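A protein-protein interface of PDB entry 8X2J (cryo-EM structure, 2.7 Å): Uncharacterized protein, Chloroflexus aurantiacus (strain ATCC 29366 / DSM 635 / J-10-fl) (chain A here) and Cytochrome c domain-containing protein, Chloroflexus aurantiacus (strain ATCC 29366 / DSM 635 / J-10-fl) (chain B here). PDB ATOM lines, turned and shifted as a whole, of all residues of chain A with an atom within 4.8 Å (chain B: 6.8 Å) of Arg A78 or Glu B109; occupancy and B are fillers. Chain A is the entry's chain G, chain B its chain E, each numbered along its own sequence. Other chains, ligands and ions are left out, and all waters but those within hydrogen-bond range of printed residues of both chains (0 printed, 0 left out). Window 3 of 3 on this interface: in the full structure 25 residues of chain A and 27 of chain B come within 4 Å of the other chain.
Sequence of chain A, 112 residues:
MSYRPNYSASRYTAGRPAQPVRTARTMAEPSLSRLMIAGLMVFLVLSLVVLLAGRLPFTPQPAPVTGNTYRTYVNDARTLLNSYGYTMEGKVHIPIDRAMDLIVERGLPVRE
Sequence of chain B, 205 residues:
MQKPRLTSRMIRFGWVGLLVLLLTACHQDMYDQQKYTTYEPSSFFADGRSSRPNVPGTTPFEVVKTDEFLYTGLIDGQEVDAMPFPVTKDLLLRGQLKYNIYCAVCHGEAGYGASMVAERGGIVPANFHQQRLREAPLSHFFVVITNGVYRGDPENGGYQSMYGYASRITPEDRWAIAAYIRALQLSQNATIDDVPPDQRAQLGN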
ATOM      1  N   VAL A  74      24.330  16.396   3.570  1.00  0.00           N
ATOM      2  CA  VAL A  74      25.022  16.055   2.330  1.00  0.00           C
ATOM      3  C   VAL A  74      24.836  14.579   1.992  1.00  0.00           C
ATOM      4  O   VAL A  74      24.548  14.227   0.841  1.00  0.00           O
ATOM      5  CB  VAL A  74      26.508  16.451   2.441  1.00  0.00           C
ATOM      6  CG1 VAL A  74      27.368  15.717   1.428  1.00  0.00           C
ATOM      7  CG2 VAL A  74      26.657  17.949   2.258  1.00  0.00           C
ATOM      8  N   ASN A  75      24.946  13.698   2.994  1.00  0.00           N
ATOM      9  CA  ASN A  75      24.775  12.267   2.761  1.00  0.00           C
ATOM     10  C   ASN A  75      23.333  11.921   2.408  1.00  0.00           C
ATOM     11  O   ASN A  75      23.096  11.081   1.532  1.00  0.00           O
ATOM     12  CB  ASN A  75      25.232  11.484   3.990  1.00  0.00           C
ATOM     13  CG  ASN A  75      26.732  11.533   4.186  1.00  0.00           C
ATOM     14  OD1 ASN A  75      27.462  12.057   3.345  1.00  0.00           O
ATOM     15  ND2 ASN A  75      27.201  10.998   5.307  1.00  0.00           N
ATOM     16  N   ASP A  76      22.359  12.572   3.059  1.00  0.00           N
ATOM     17  CA  ASP A  76      20.957  12.339   2.723  1.00  0.00           C
ATOM     18  C   ASP A  76      20.628  12.831   1.319  1.00  0.00           C
ATOM     19  O   ASP A  76      19.897  12.161   0.579  1.00  0.00           O
ATOM     20  CB  ASP A  76      20.053  13.015   3.754  1.00  0.00           C
ATOM     21  CG  ASP A  76      19.970  12.240   5.052  1.00  0.00           C
ATOM     22  OD1 ASP A  76      20.493  11.108   5.106  1.00  0.00           O
ATOM     23  OD2 ASP A  76      19.383  12.765   6.021  1.00  0.00           O
ATOM     24  N   ALA A  77      21.181  13.982   0.922  1.00  0.00           N
ATOM     25  CA  ALA A  77      20.924  14.501  -0.419  1.00  0.00           C
ATOM     26  C   ALA A  77      21.606  13.657  -1.489  1.00  0.00           C
ATOM     27  O   ALA A  77      21.050  13.458  -2.575  1.00  0.00           O
ATOM     28  CB  ALA A  77      21.377  15.956  -0.509  1.00  0.00           C
ATOM     29  N   ARG A  78      22.805  13.140  -1.203  1.00  0.00           N
ATOM     30  CA  ARG A  78      23.486  12.289  -2.173  1.00  0.00           C
ATOM     31  C   ARG A  78      22.842  10.910  -2.264  1.00  0.00           C
ATOM     32  O   ARG A  78      22.898  10.274  -3.322  1.00  0.00           O
ATOM     33  CB  ARG A  78      24.966  12.163  -1.818  1.00  0.00           C
ATOM     34  CG  ARG A  78      25.781  13.410  -2.120  1.00  0.00           C
ATOM     35  CD  ARG A  78      27.269  13.134  -2.004  1.00  0.00           C
ATOM     36  NE  ARG A  78      28.027  14.327  -1.645  1.00  0.00           N
ATOM     37  CZ  ARG A  78      28.458  15.235  -2.510  1.00  0.00           C
ATOM     38  NH1 ARG A  78      28.208  15.130  -3.805  1.00  0.00           N
ATOM     39  NH2 ARG A  78      29.159  16.274  -2.066  1.00  0.00           N
ATOM     40  N   THR A  79      22.236  10.429  -1.174  1.00  0.00           N
ATOM     41  CA  THR A  79      21.455   9.200  -1.252  1.00  0.00           C
ATOM     42  C   THR A  79      20.156   9.421  -2.020  1.00  0.00           C
ATOM     43  O   THR A  79      19.722   8.549  -2.780  1.00  0.00           O
ATOM     44  CB  THR A  79      21.165   8.669   0.152  1.00  0.00           C
ATOM     45  OG1 THR A  79      22.343   8.786   0.960  1.00  0.00           O
ATOM     46  CG2 THR A  79      20.742   7.209   0.096  1.00  0.00           C
ATOM     47  N   LEU A  80      19.523  10.585  -1.838  1.00  0.00           N
ATOM     48  CA  LEU A  80      18.298  10.891  -2.565  1.00  0.00           C
ATOM     49  C   LEU A  80      18.557  11.190  -4.035  1.00  0.00           C
ATOM     50  O   LEU A  80      17.638  11.067  -4.853  1.00  0.00           O
ATOM     51  CB  LEU A  80      17.583  12.074  -1.909  1.00  0.00           C
ATOM     52  CG  LEU A  80      16.072  12.177  -2.124  1.00  0.00           C
ATOM     53  CD1 LEU A  80      15.345  11.101  -1.330  1.00  0.00           C
ATOM     54  CD2 LEU A  80      15.566  13.561  -1.744  1.00  0.00           C
ATOM     55  N   LEU A  81      19.780  11.575  -4.391  1.00  0.00           N
ATOM     56  CA  LEU A  81      20.138  11.862  -5.771  1.00  0.00           C
ATOM     57  C   LEU A  81      20.654  10.637  -6.514  1.00  0.00           C
ATOM     58  O   LEU A  81      21.134  10.772  -7.644  1.00  0.00           O
ATOM     59  CB  LEU A  81      21.182  12.979  -5.824  1.00  0.00           C
ATOM     60  CG  LEU A  81      20.656  14.414  -5.763  1.00  0.00           C
ATOM     61  CD1 LEU A  81      21.794  15.408  -5.929  1.00  0.00           C
ATOM     62  CD2 LEU A  81      19.577  14.644  -6.808  1.00  0.00           C
ATOM     63  N   ASN A  82      20.578   9.453  -5.907  1.00  0.00           N
ATOM     64  CA  ASN A  82      21.025   8.220  -6.537  1.00  0.00           C
ATOM     65  C   ASN A  82      20.040   7.104  -6.219  1.00  0.00           C
ATOM     66  O   ASN A  82      19.151   7.252  -5.374  1.00  0.00           O
ATOM     67  CB  ASN A  82      22.438   7.833  -6.080  1.00  0.00           C
ATOM     68  CG  ASN A  82      23.511   8.717  -6.681  1.00  0.00           C
ATOM     69  OD1 ASN A  82      23.477   9.034  -7.870  1.00  0.00           O
ATOM     70  ND2 ASN A  82      24.474   9.119  -5.862  1.00  0.00           N
ATOM     71  N   GLN B  96      27.048  21.720 -12.109  1.00  0.00           N
ATOM     72  CA  GLN B  96      26.953  20.914 -10.896  1.00  0.00           C
ATOM     73  C   GLN B  96      28.068  21.257  -9.917  1.00  0.00           C
ATOM     74  O   GLN B  96      27.829  21.376  -8.708  1.00  0.00           O
ATOM     75  CB  GLN B  96      26.994  19.428 -11.250  1.00  0.00           C
ATOM     76  CG  GLN B  96      26.982  18.496 -10.049  1.00  0.00           C
ATOM     77  CD  GLN B  96      27.188  17.047 -10.428  1.00  0.00           C
ATOM     78  OE1 GLN B  96      27.616  16.737 -11.537  1.00  0.00           O
ATOM     79  NE2 GLN B  96      26.880  16.146  -9.503  1.00  0.00           N
ATOM     80  N   TYR B  99      27.353  24.745  -8.527  1.00  0.00           N
ATOM     81  CA  TYR B  99      26.237  24.625  -7.595  1.00  0.00           C
ATOM     82  C   TYR B  99      26.696  24.049  -6.263  1.00  0.00           C
ATOM     83  O   TYR B  99      26.258  24.504  -5.200  1.00  0.00           O
ATOM     84  CB  TYR B  99      25.141  23.751  -8.211  1.00  0.00           C
ATOM     85  CG  TYR B  99      23.951  23.495  -7.309  1.00  0.00           C
ATOM     86  CD1 TYR B  99      22.905  24.400  -7.245  1.00  0.00           C
ATOM     87  CD2 TYR B  99      23.861  22.335  -6.544  1.00  0.00           C
ATOM     88  CE1 TYR B  99      21.824  24.183  -6.422  1.00  0.00           C
ATOM     89  CE2 TYR B  99      22.781  22.107  -5.723  1.00  0.00           C
ATOM     90  CZ  TYR B  99      21.765  23.033  -5.670  1.00  0.00           C
ATOM     91  OH  TYR B  99      20.685  22.809  -4.856  1.00  0.00           O
ATOM     92  N   ASN B 100      27.555  23.025  -6.302  1.00  0.00           N
ATOM     93  CA  ASN B 100      28.051  22.433  -5.066  1.00  0.00           C
ATOM     94  C   ASN B 100      28.983  23.381  -4.322  1.00  0.00           C
ATOM     95  O   ASN B 100      29.064  23.327  -3.090  1.00  0.00           O
ATOM     96  CB  ASN B 100      28.760  21.113  -5.363  1.00  0.00           C
ATOM     97  CG  ASN B 100      27.808  20.037  -5.844  1.00  0.00           C
ATOM     98  OD1 ASN B 100      26.623  20.287  -6.045  1.00  0.00           O
ATOM     99  ND2 ASN B 100      28.328  18.831  -6.036  1.00  0.00           N
ATOM    100  N   ILE B 101      29.687  24.249  -5.046  1.00  0.00           N
ATOM    101  CA  ILE B 101      30.558  25.224  -4.396  1.00  0.00           C
ATOM    102  C   ILE B 101      29.741  26.350  -3.771  1.00  0.00           C
ATOM    103  O   ILE B 101      29.849  26.625  -2.571  1.00  0.00           O
ATOM    104  CB  ILE B 101      31.592  25.775  -5.394  1.00  0.00           C
ATOM    105  CG1 ILE B 101      32.644  24.721  -5.720  1.00  0.00           C
ATOM    106  CG2 ILE B 101      32.275  27.002  -4.830  1.00  0.00           C
ATOM    107  CD1 ILE B 101      33.313  24.950  -7.047  1.00  0.00           C
ATOM    108  N   CYS B 103      26.110  27.227  -4.183  1.00  0.00           N
ATOM    109  CA  CYS B 103      24.668  27.252  -3.986  1.00  0.00           C
ATOM    110  C   CYS B 103      24.145  26.155  -3.077  1.00  0.00           C
ATOM    111  O   CYS B 103      23.088  26.329  -2.471  1.00  0.00           O
ATOM    112  CB  CYS B 103      23.952  27.148  -5.334  1.00  0.00           C
ATOM    113  SG  CYS B 103      24.686  28.123  -6.654  1.00  0.00           S
ATOM    114  N   ALA B 104      24.854  25.035  -2.961  1.00  0.00           N
ATOM    115  CA  ALA B 104      24.383  23.905  -2.172  1.00  0.00           C
ATOM    116  C   ALA B 104      24.622  24.077  -0.679  1.00  0.00           C
ATOM    117  O   ALA B 104      24.222  23.203   0.098  1.00  0.00           O
ATOM    118  CB  ALA B 104      25.048  22.614  -2.654  1.00  0.00           C
ATOM    119  N   VAL B 105      25.275  25.165  -0.266  1.00  0.00           N
ATOM    120  CA  VAL B 105      25.499  25.417   1.154  1.00  0.00           C
ATOM    121  C   VAL B 105      24.184  25.744   1.851  1.00  0.00           C
ATOM    122  O   VAL B 105      23.922  25.279   2.967  1.00  0.00           O
ATOM    123  CB  VAL B 105      26.538  26.539   1.327  1.00  0.00           C
ATOM    124  CG1 VAL B 105      26.830  26.788   2.793  1.00  0.00           C
ATOM    125  CG2 VAL B 105      27.813  26.197   0.576  1.00  0.00           C
ATOM    126  N   CYS B 106      23.326  26.530   1.201  1.00  0.00           N
ATOM    127  CA  CYS B 106      22.026  26.896   1.748  1.00  0.00           C
ATOM    128  C   CYS B 106      20.886  26.082   1.149  1.00  0.00           C
ATOM    129  O   CYS B 106      20.064  25.531   1.886  1.00  0.00           O
ATOM    130  CB  CYS B 106      21.761  28.388   1.524  1.00  0.00           C
ATOM    131  SG  CYS B 106      22.823  29.487   2.473  1.00  0.00           S
ATOM    132  N   HIS B 107      20.816  25.995  -0.180  1.00  0.00           N
ATOM    133  CA  HIS B 107      19.722  25.300  -0.846  1.00  0.00           C
ATOM    134  C   HIS B 107      19.841  23.783  -0.782  1.00  0.00           C
ATOM    135  O   HIS B 107      18.866  23.091  -1.090  1.00  0.00           O
ATOM    136  CB  HIS B 107      19.631  25.741  -2.309  1.00  0.00           C
ATOM    137  CG  HIS B 107      19.223  27.171  -2.490  1.00  0.00           C
ATOM    138  ND1 HIS B 107      17.907  27.560  -2.614  1.00  0.00           N
ATOM    139  CD2 HIS B 107      19.959  28.303  -2.583  1.00  0.00           C
ATOM    140  CE1 HIS B 107      17.849  28.871  -2.766  1.00  0.00           C
ATOM    141  NE2 HIS B 107      19.081  29.347  -2.753  1.00  0.00           N
ATOM    142  N   GLY B 108      20.994  23.251  -0.394  1.00  0.00           N
ATOM    143  CA  GLY B 108      21.198  21.820  -0.347  1.00  0.00           C
ATOM    144  C   GLY B 108      21.715  21.265  -1.663  1.00  0.00           C
ATOM    145  O   GLY B 108      21.641  21.898  -2.715  1.00  0.00           O
ATOM    146  N   GLU B 109      22.265  20.049  -1.586  1.00  0.00           N
ATOM    147  CA  GLU B 109      22.768  19.388  -2.786  1.00  0.00           C
ATOM    148  C   GLU B 109      21.627  18.941  -3.691  1.00  0.00           C
ATOM    149  O   GLU B 109      21.711  19.075  -4.917  1.00  0.00           O
ATOM    150  CB  GLU B 109      23.645  18.196  -2.403  1.00  0.00           C
ATOM    151  CG  GLU B 109      24.881  18.552  -1.596  1.00  0.00           C
ATOM    152  CD  GLU B 109      26.120  18.681  -2.456  1.00  0.00           C
ATOM    153  OE1 GLU B 109      26.037  18.385  -3.665  1.00  0.00           O
ATOM    154  OE2 GLU B 109      27.179  19.070  -1.922  1.00  0.00           O
ATOM    155  N   ALA B 110      20.555  18.407  -3.107  1.00  0.00           N
ATOM    156  CA  ALA B 110      19.388  18.001  -3.877  1.00  0.00           C
ATOM    157  C   ALA B 110      18.471  19.165  -4.219  1.00  0.00           C
ATOM    158  O   ALA B 110      17.599  19.013  -5.080  1.00  0.00           O
ATOM    159  CB  ALA B 110      18.596  16.935  -3.117  1.00  0.00           C
ATOM    160  N   GLY B 111      18.644  20.314  -3.572  1.00  0.00           N
ATOM    161  CA  GLY B 111      17.853  21.485  -3.881  1.00  0.00           C
ATOM    162  C   GLY B 111      16.564  21.631  -3.113  1.00  0.00           C
ATOM    163  O   GLY B 111      15.708  22.422  -3.520  1.00  0.00           O
ATOM    164  N   TYR B 112      16.395  20.907  -2.012  1.00  0.00           N
ATOM    165  CA  TYR B 112      15.159  20.955  -1.244  1.00  0.00           C
ATOM    166  C   TYR B 112      15.154  22.048  -0.185  1.00  0.00           C
ATOM    167  O   TYR B 112      14.165  22.179   0.543  1.00  0.00           O
ATOM    168  CB  TYR B 112      14.893  19.598  -0.590  1.00  0.00           C
ATOM    169  CG  TYR B 112      14.145  18.637  -1.482  1.00  0.00           C
ATOM    170  CD1 TYR B 112      12.759  18.688  -1.583  1.00  0.00           C
ATOM    171  CD2 TYR B 112      14.823  17.683  -2.232  1.00  0.00           C
ATOM    172  CE1 TYR B 112      12.070  17.812  -2.401  1.00  0.00           C
ATOM    173  CE2 TYR B 112      14.142  16.802  -3.051  1.00  0.00           C
ATOM    174  CZ  TYR B 112      12.766  16.873  -3.131  1.00  0.00           C
ATOM    175  OH  TYR B 112      12.084  16.001  -3.946  1.00  0.00           O
ATOM    176  N   ALA B 114      16.960  22.224   2.521  1.00  0.00           N
ATOM    177  CA  ALA B 114      17.293  21.717   3.845  1.00  0.00           C
ATOM    178  C   ALA B 114      18.807  21.675   3.990  1.00  0.00           C
ATOM    179  O   ALA B 114      19.481  20.928   3.273  1.00  0.00           O
ATOM    180  CB  ALA B 114      16.692  20.330   4.067  1.00  0.00           C
ATOM    181  N   SER B 115      19.336  22.473   4.915  1.00  0.00           N
ATOM    182  CA  SER B 115      20.775  22.553   5.120  1.00  0.00           C
ATOM    183  C   SER B 115      21.052  23.066   6.526  1.00  0.00           C
ATOM    184  O   SER B 115      20.148  23.506   7.242  1.00  0.00           O
ATOM    185  CB  SER B 115      21.439  23.447   4.073  1.00  0.00           C
ATOM    186  OG  SER B 115      21.055  24.798   4.239  1.00  0.00           O
ATOM    187  N   TYR B 180      21.947  23.366 -14.400  1.00  0.00           N
ATOM    188  CA  TYR B 180      21.931  22.317 -13.383  1.00  0.00           C
ATOM    189  C   TYR B 180      20.704  22.415 -12.481  1.00  0.00           C
ATOM    190  O   TYR B 180      20.257  21.398 -11.942  1.00  0.00           O
ATOM    191  CB  TYR B 180      23.206  22.359 -12.544  1.00  0.00           C
ATOM    192  CG  TYR B 180      23.320  21.174 -11.614  1.00  0.00           C
ATOM    193  CD1 TYR B 180      23.361  19.877 -12.111  1.00  0.00           C
ATOM    194  CD2 TYR B 180      23.343  21.350 -10.237  1.00  0.00           C
ATOM    195  CE1 TYR B 180      23.445  18.790 -11.263  1.00  0.00           C
ATOM    196  CE2 TYR B 180      23.433  20.270  -9.382  1.00  0.00           C
ATOM    197  CZ  TYR B 180      23.481  18.995  -9.899  1.00  0.00           C
ATOM    198  OH  TYR B 180      23.569  17.922  -9.044  1.00  0.00           O
ATOM    199  N   LEU B 184      18.234  19.389 -11.848  1.00  0.00           N
ATOM    200  CA  LEU B 184      17.744  18.946 -10.542  1.00  0.00           C
ATOM    201  C   LEU B 184      16.220  18.930 -10.496  1.00  0.00           C
ATOM    202  O   LEU B 184      15.620  18.070  -9.835  1.00  0.00           O
ATOM    203  CB  LEU B 184      18.292  19.850  -9.439  1.00  0.00           C
ATOM    204  CG  LEU B 184      19.705  19.599  -8.914  1.00  0.00           C
ATOM    205  CD1 LEU B 184      20.111  20.725  -7.982  1.00  0.00           C
ATOM    206  CD2 LEU B 184      19.789  18.259  -8.204  1.00  0.00           C
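The side-chain carboxylate of Glu B109 is in salt-bridge range of the guanidinium group of Arg A78 (3.4 Å).
The side-chain carboxylate of Glu B109 sits close to the side-chain amide oxygen of Asn B100 (3.1 Å).
The backbone NH of Tyr B112 sits at hydrogen-bond distance from the backbone carbonyl oxygen of His B107 (3.4 Å).
ND2 of Asn A82 lies within hydrogen-bond range of O of Arg A78 (3.2 Å).
Ala A77 touches Glu B109.
Ala B110 touches Ala A77.
Leu A80 touches Tyr B112 (CD2 to CE2, 3.8 Å).
Leu A81 touches Glu B109 (CD1 to O, 3.8 Å).
Leu A81 touches Leu B184 (CD2 to CD2, 3.9 Å).
Printed residues of chain B within 4 Å of Ala A77: Glu B109 (3.7 Å) and Ala B110 (3.7 Å).
Of the printed residues of chain B, Leu A80 touches Tyr B112 (3.8 Å).
Printed residues of chain B within 4 Å of Leu A81: Glu B109 (3.8 Å) and Leu B184 (3.9 Å).
Of chain A, only Ala A77 (3.7 Å), Arg A78 (3.4 Å) and Leu A81 (3.8 Å) come within 4 Å of Glu B109.
Printed residues of chain A within 4 Å of Leu B184: Leu A81.
The nearest residue of chain B that does not touch Arg A78 is Asn B100 (4.3 Å).
Hydrophobic or aromatic side chains of chain B within 4 Å of the printed part of chain A: Ala B110, Tyr B112 and Leu B184.
Of the 9 printed residues of chain A, 4 touch a printed residue of chain B.
Printed residues of chain A that touch a printed residue of chain B: Ala A77, Arg A78, Leu A80 and Leu A81.
Hydrophobic or aromatic side chains of chain A within 4 Å of the printed part of chain B: Ala A77, Leu A80 and Leu A81.
Along chain A the printed residues that touch a printed residue of chain B span positions 77 to 81.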
